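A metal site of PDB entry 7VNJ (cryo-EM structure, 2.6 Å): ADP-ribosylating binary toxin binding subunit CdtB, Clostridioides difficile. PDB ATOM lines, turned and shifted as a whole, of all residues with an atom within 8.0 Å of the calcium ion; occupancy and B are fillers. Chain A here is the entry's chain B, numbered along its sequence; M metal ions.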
ATOM      1  N   PHE A 418     -19.516   9.311 -18.695  1.00  0.00           N
ATOM      2  CA  PHE A 418     -20.842   9.326 -18.104  1.00  0.00           C
ATOM      3  C   PHE A 418     -20.916   8.307 -16.987  1.00  0.00           C
ATOM      4  O   PHE A 418     -20.360   7.206 -17.085  1.00  0.00           O
ATOM      5  CB  PHE A 418     -21.911   9.017 -19.172  1.00  0.00           C
ATOM      6  CG  PHE A 418     -23.259   8.677 -18.604  1.00  0.00           C
ATOM      7  CD1 PHE A 418     -24.116   9.685 -18.179  1.00  0.00           C
ATOM      8  CD2 PHE A 418     -23.669   7.365 -18.507  1.00  0.00           C
ATOM      9  CE1 PHE A 418     -25.356   9.376 -17.665  1.00  0.00           C
ATOM     10  CE2 PHE A 418     -24.917   7.050 -17.992  1.00  0.00           C
ATOM     11  CZ  PHE A 418     -25.752   8.063 -17.567  1.00  0.00           C
ATOM     12  N   THR A 419     -21.605   8.671 -15.911  1.00  0.00           N
ATOM     13  CA  THR A 419     -21.872   7.770 -14.805  1.00  0.00           C
ATOM     14  C   THR A 419     -23.299   7.963 -14.317  1.00  0.00           C
ATOM     15  O   THR A 419     -23.805   9.088 -14.274  1.00  0.00           O
ATOM     16  CB  THR A 419     -20.886   7.971 -13.651  1.00  0.00           C
ATOM     17  OG1 THR A 419     -21.174   7.037 -12.600  1.00  0.00           O
ATOM     18  CG2 THR A 419     -20.968   9.396 -13.103  1.00  0.00           C
ATOM     19  N   ASN A 420     -23.958   6.852 -13.986  1.00  0.00           N
ATOM     20  CA  ASN A 420     -25.296   6.879 -13.408  1.00  0.00           C
ATOM     21  C   ASN A 420     -25.295   6.520 -11.940  1.00  0.00           C
ATOM     22  O   ASN A 420     -26.360   6.533 -11.312  1.00  0.00           O
ATOM     23  CB  ASN A 420     -26.229   5.937 -14.182  1.00  0.00           C
ATOM     24  CG  ASN A 420     -25.694   4.523 -14.252  1.00  0.00           C
ATOM     25  OD1 ASN A 420     -24.516   4.281 -13.976  1.00  0.00           O
ATOM     26  ND2 ASN A 420     -26.555   3.581 -14.607  1.00  0.00           N
ATOM     27  N   PHE A 421     -24.136   6.191 -11.374  1.00  0.00           N
ATOM     28  CA  PHE A 421     -23.933   5.786  -9.986  1.00  0.00           C
ATOM     29  C   PHE A 421     -24.567   4.443  -9.656  1.00  0.00           C
ATOM     30  O   PHE A 421     -24.696   4.101  -8.479  1.00  0.00           O
ATOM     31  CB  PHE A 421     -24.456   6.842  -8.996  1.00  0.00           C
ATOM     32  CG  PHE A 421     -23.810   8.186  -9.139  1.00  0.00           C
ATOM     33  CD1 PHE A 421     -22.429   8.312  -9.195  1.00  0.00           C
ATOM     34  CD2 PHE A 421     -24.575   9.330  -9.209  1.00  0.00           C
ATOM     35  CE1 PHE A 421     -21.831   9.541  -9.322  1.00  0.00           C
ATOM     36  CE2 PHE A 421     -23.990  10.574  -9.341  1.00  0.00           C
ATOM     37  CZ  PHE A 421     -22.618  10.679  -9.402  1.00  0.00           C
ATOM     38  N   ASP A 422     -24.977   3.671 -10.660  1.00  0.00           N
ATOM     39  CA  ASP A 422     -25.523   2.329 -10.429  1.00  0.00           C
ATOM     40  C   ASP A 422     -24.639   1.243 -11.008  1.00  0.00           C
ATOM     41  O   ASP A 422     -24.135   0.393 -10.273  1.00  0.00           O
ATOM     42  CB  ASP A 422     -26.930   2.232 -11.033  1.00  0.00           C
ATOM     43  CG  ASP A 422     -27.892   3.212 -10.421  1.00  0.00           C
ATOM     44  OD1 ASP A 422     -27.965   4.350 -10.926  1.00  0.00           O
ATOM     45  OD2 ASP A 422     -28.591   2.844  -9.457  1.00  0.00           O
ATOM     46  N   ASP A 423     -24.435   1.232 -12.327  1.00  0.00           N
ATOM     47  CA  ASP A 423     -23.640   0.200 -12.967  1.00  0.00           C
ATOM     48  C   ASP A 423     -22.696   0.706 -14.046  1.00  0.00           C
ATOM     49  O   ASP A 423     -21.806  -0.045 -14.452  1.00  0.00           O
ATOM     50  CB  ASP A 423     -24.563  -0.859 -13.585  1.00  0.00           C
ATOM     51  CG  ASP A 423     -25.536  -0.275 -14.589  1.00  0.00           C
ATOM     52  OD1 ASP A 423     -25.626   0.964 -14.675  1.00  0.00           O
ATOM     53  OD2 ASP A 423     -26.200  -1.060 -15.304  1.00  0.00           O
ATOM     54  N   THR A 436     -23.795   5.490  -2.589  1.00  0.00           N
ATOM     55  CA  THR A 436     -24.876   5.125  -3.510  1.00  0.00           C
ATOM     56  C   THR A 436     -25.735   4.024  -2.914  1.00  0.00           C
ATOM     57  O   THR A 436     -26.109   3.054  -3.575  1.00  0.00           O
ATOM     58  CB  THR A 436     -24.307   4.685  -4.863  1.00  0.00           C
ATOM     59  OG1 THR A 436     -23.342   3.653  -4.655  1.00  0.00           O
ATOM     60  CG2 THR A 436     -23.633   5.859  -5.550  1.00  0.00           C
ATOM     61  N   ASN A 438     -28.724   4.696  -1.419  1.00  0.00           N
ATOM     62  CA  ASN A 438     -30.083   5.207  -1.330  1.00  0.00           C
ATOM     63  C   ASN A 438     -30.798   5.003  -2.653  1.00  0.00           C
ATOM     64  O   ASN A 438     -30.189   5.104  -3.730  1.00  0.00           O
ATOM     65  CB  ASN A 438     -30.089   6.685  -0.945  1.00  0.00           C
ATOM     66  CG  ASN A 438     -29.309   7.540  -1.917  1.00  0.00           C
ATOM     67  OD1 ASN A 438     -28.402   7.063  -2.600  1.00  0.00           O
ATOM     68  ND2 ASN A 438     -29.660   8.820  -1.998  1.00  0.00           N
ATOM     69  N   ASP A 440     -32.542   6.708  -4.703  1.00  0.00           N
ATOM     70  CA  ASP A 440     -32.901   8.037  -5.211  1.00  0.00           C
ATOM     71  C   ASP A 440     -32.283   8.253  -6.586  1.00  0.00           C
ATOM     72  O   ASP A 440     -31.773   7.314  -7.204  1.00  0.00           O
ATOM     73  CB  ASP A 440     -32.448   9.125  -4.245  1.00  0.00           C
ATOM     74  CG  ASP A 440     -33.376  10.326  -4.257  1.00  0.00           C
ATOM     75  OD1 ASP A 440     -34.353  10.314  -5.034  1.00  0.00           O
ATOM     76  OD2 ASP A 440     -33.119  11.285  -3.496  1.00  0.00           O
ATOM     77  N   GLY A 441     -32.346   9.479  -7.092  1.00  0.00           N
ATOM     78  CA  GLY A 441     -31.839   9.765  -8.419  1.00  0.00           C
ATOM     79  C   GLY A 441     -32.829   9.386  -9.496  1.00  0.00           C
ATOM     80  O   GLY A 441     -33.936   8.908  -9.240  1.00  0.00           O
ATOM     81  N   LEU A 442     -32.412   9.623 -10.743  1.00  0.00           N
ATOM     82  CA  LEU A 442     -33.256   9.242 -11.872  1.00  0.00           C
ATOM     83  C   LEU A 442     -33.497   7.738 -11.902  1.00  0.00           C
ATOM     84  O   LEU A 442     -34.613   7.290 -12.172  1.00  0.00           O
ATOM     85  CB  LEU A 442     -32.623   9.716 -13.178  1.00  0.00           C
ATOM     86  CG  LEU A 442     -32.972  11.146 -13.598  1.00  0.00           C
ATOM     87  CD1 LEU A 442     -32.091  11.626 -14.726  1.00  0.00           C
ATOM     88  CD2 LEU A 442     -34.422  11.184 -14.033  1.00  0.00           C
ATOM     89  N   GLN A 443     -32.463   6.941 -11.627  1.00  0.00           N
ATOM     90  CA  GLN A 443     -32.616   5.491 -11.541  1.00  0.00           C
ATOM     91  C   GLN A 443     -31.786   4.977 -10.357  1.00  0.00           C
ATOM     92  O   GLN A 443     -30.628   4.598 -10.523  1.00  0.00           O
ATOM     93  CB  GLN A 443     -32.205   4.819 -12.844  1.00  0.00           C
ATOM     94  CG  GLN A 443     -33.202   4.998 -13.982  1.00  0.00           C
ATOM     95  CD  GLN A 443     -32.764   6.041 -14.991  1.00  0.00           C
ATOM     96  OE1 GLN A 443     -31.574   6.277 -15.179  1.00  0.00           O
ATOM     97  NE2 GLN A 443     -33.726   6.675 -15.644  1.00  0.00           N
ATOM     98  N   GLY A 444     -32.409   4.962  -9.179  1.00  0.00           N
ATOM     99  CA  GLY A 444     -31.901   4.195  -8.052  1.00  0.00           C
ATOM    100  C   GLY A 444     -30.510   4.524  -7.560  1.00  0.00           C
ATOM    101  O   GLY A 444     -29.826   3.650  -7.037  1.00  0.00           O
ATOM    102  N   SER A 445     -30.073   5.777  -7.702  1.00  0.00           N
ATOM    103  CA  SER A 445     -28.777   6.188  -7.164  1.00  0.00           C
ATOM    104  C   SER A 445     -28.669   7.701  -7.227  1.00  0.00           C
ATOM    105  O   SER A 445     -29.048   8.308  -8.223  1.00  0.00           O
ATOM    106  CB  SER A 445     -27.614   5.560  -7.938  1.00  0.00           C
ATOM    107  OG  SER A 445     -27.588   6.007  -9.283  1.00  0.00           O
ATOM    108  N   ALA A 446     -28.140   8.297  -6.161  1.00  0.00           N
ATOM    109  CA  ALA A 446     -27.973   9.741  -6.089  1.00  0.00           C
ATOM    110  C   ALA A 446     -26.526  10.159  -5.885  1.00  0.00           C
ATOM    111  O   ALA A 446     -26.029  11.029  -6.618  1.00  0.00           O
ATOM    112  CB  ALA A 446     -28.843  10.317  -4.964  1.00  0.00           C
ATOM    113  N   ASN A 447     -25.829   9.565  -4.916  1.00  0.00           N
ATOM    114  CA  ASN A 447     -24.435   9.905  -4.612  1.00  0.00           C
ATOM    115  C   ASN A 447     -24.277  11.389  -4.293  1.00  0.00           C
ATOM    116  O   ASN A 447     -23.595  12.138  -5.004  1.00  0.00           O
ATOM    117  CB  ASN A 447     -23.505   9.479  -5.752  1.00  0.00           C
ATOM    118  CG  ASN A 447     -22.039   9.499  -5.341  1.00  0.00           C
ATOM    119  OD1 ASN A 447     -21.550   8.551  -4.717  1.00  0.00           O
ATOM    120  ND2 ASN A 447     -21.341  10.577  -5.671  1.00  0.00           N
ATOM    121  N   TYR A 503     -36.545  16.821 -10.955  1.00  0.00           N
ATOM    122  CA  TYR A 503     -35.263  16.715 -11.639  1.00  0.00           C
ATOM    123  C   TYR A 503     -35.205  17.677 -12.814  1.00  0.00           C
ATOM    124  O   TYR A 503     -36.116  17.701 -13.649  1.00  0.00           O
ATOM    125  CB  TYR A 503     -35.046  15.274 -12.124  1.00  0.00           C
ATOM    126  CG  TYR A 503     -34.802  14.289 -11.008  1.00  0.00           C
ATOM    127  CD1 TYR A 503     -34.436  14.718  -9.752  1.00  0.00           C
ATOM    128  CD2 TYR A 503     -34.986  12.926 -11.205  1.00  0.00           C
ATOM    129  CE1 TYR A 503     -34.217  13.828  -8.735  1.00  0.00           C
ATOM    130  CE2 TYR A 503     -34.775  12.030 -10.186  1.00  0.00           C
ATOM    131  CZ  TYR A 503     -34.390  12.483  -8.946  1.00  0.00           C
ATOM    132  OH  TYR A 503     -34.185  11.616  -7.904  1.00  0.00           O
ATOM    133  N   LEU A 532     -28.023  14.591  -6.866  1.00  0.00           N
ATOM    134  CA  LEU A 532     -27.466  14.598  -8.200  1.00  0.00           C
ATOM    135  C   LEU A 532     -27.642  13.226  -8.840  1.00  0.00           C
ATOM    136  O   LEU A 532     -27.856  12.229  -8.150  1.00  0.00           O
ATOM    137  CB  LEU A 532     -25.977  14.991  -8.194  1.00  0.00           C
ATOM    138  CG  LEU A 532     -25.645  16.454  -7.932  1.00  0.00           C
ATOM    139  CD1 LEU A 532     -24.143  16.653  -7.813  1.00  0.00           C
ATOM    140  CD2 LEU A 532     -26.215  17.340  -9.021  1.00  0.00           C
ATOM    141  N   ASP A 533     -27.561  13.191 -10.170  1.00  0.00           N
ATOM    142  CA  ASP A 533     -27.593  11.944 -10.916  1.00  0.00           C
ATOM    143  C   ASP A 533     -27.216  12.196 -12.356  1.00  0.00           C
ATOM    144  O   ASP A 533     -27.404  13.301 -12.879  1.00  0.00           O
ATOM    145  CB  ASP A 533     -28.969  11.267 -10.853  1.00  0.00           C
ATOM    146  CG  ASP A 533     -28.890   9.762 -10.957  1.00  0.00           C
ATOM    147  OD1 ASP A 533     -27.767   9.222 -10.990  1.00  0.00           O
ATOM    148  OD2 ASP A 533     -29.955   9.109 -10.995  1.00  0.00           O
ATOM    149  N   ASN A 534     -26.677  11.164 -13.010  1.00  0.00           N
ATOM    150  CA  ASN A 534     -26.399  11.150 -14.449  1.00  0.00           C
ATOM    151  C   ASN A 534     -25.479  12.307 -14.849  1.00  0.00           C
ATOM    152  O   ASN A 534     -25.856  13.200 -15.607  1.00  0.00           O
ATOM    153  CB  ASN A 534     -27.706  11.169 -15.243  1.00  0.00           C
ATOM    154  CG  ASN A 534     -28.441   9.859 -15.186  1.00  0.00           C
ATOM    155  OD1 ASN A 534     -27.966   8.888 -14.598  1.00  0.00           O
ATOM    156  ND2 ASN A 534     -29.615   9.800 -15.808  1.00  0.00           N
ATOM    157  N   LEU A 535     -24.264  12.277 -14.325  1.00  0.00           N
ATOM    158  CA  LEU A 535     -23.247  13.251 -14.673  1.00  0.00           C
ATOM    159  C   LEU A 535     -22.509  12.808 -15.922  1.00  0.00           C
ATOM    160  O   LEU A 535     -22.039  11.658 -15.992  1.00  0.00           O
ATOM    161  CB  LEU A 535     -22.269  13.445 -13.518  1.00  0.00           C
ATOM    162  CG  LEU A 535     -22.915  13.755 -12.167  1.00  0.00           C
ATOM    163  CD1 LEU A 535     -21.858  13.836 -11.071  1.00  0.00           C
ATOM    164  CD2 LEU A 535     -23.707  15.050 -12.236  1.00  0.00           C
HETATM  165 CA    CA M   1     -28.849   6.892 -11.135  1.00  0.00          CA
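OD2 of Asp 533 sits close to N of Gln 443 (3.4 Å). OD2 of Asp 533 lies close to N of Leu 442, 2.5 Å away. ND2 of Asn 420 is in hydrogen-bond range of OD1 of Asp 423 (2.8 Å). The side-chain carboxylate of Asp 422 sits close to the backbone carbonyl oxygen of Gln 443, at 2.7 Å.
Within 4 Å of the calcium ion: Asn 420, Asp 422, Gln 443, Ser 445 and Asp 533. Along chain A the residues within 4 Å of the calcium ion span positions 420 to 533.
The calcium ion is bound by the side-chain hydroxyl (OG) of Ser 445 (2.4 Å), the side-chain carboxylate (OD2) of Asp 533 (2.5 Å), the backbone carbonyl oxygen (O) of Asn 420 (2.5 Å), the side-chain carboxylate (OD1) of Asp 533 (2.6 Å) and the side-chain carboxylate (OD1) of Asp 422 (2.7 Å). The calcium ion has five donor atoms within binding distance. Slightly farther from the calcium ion lies the backbone carbonyl oxygen (O) of Gln 443 (3.0 Å).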
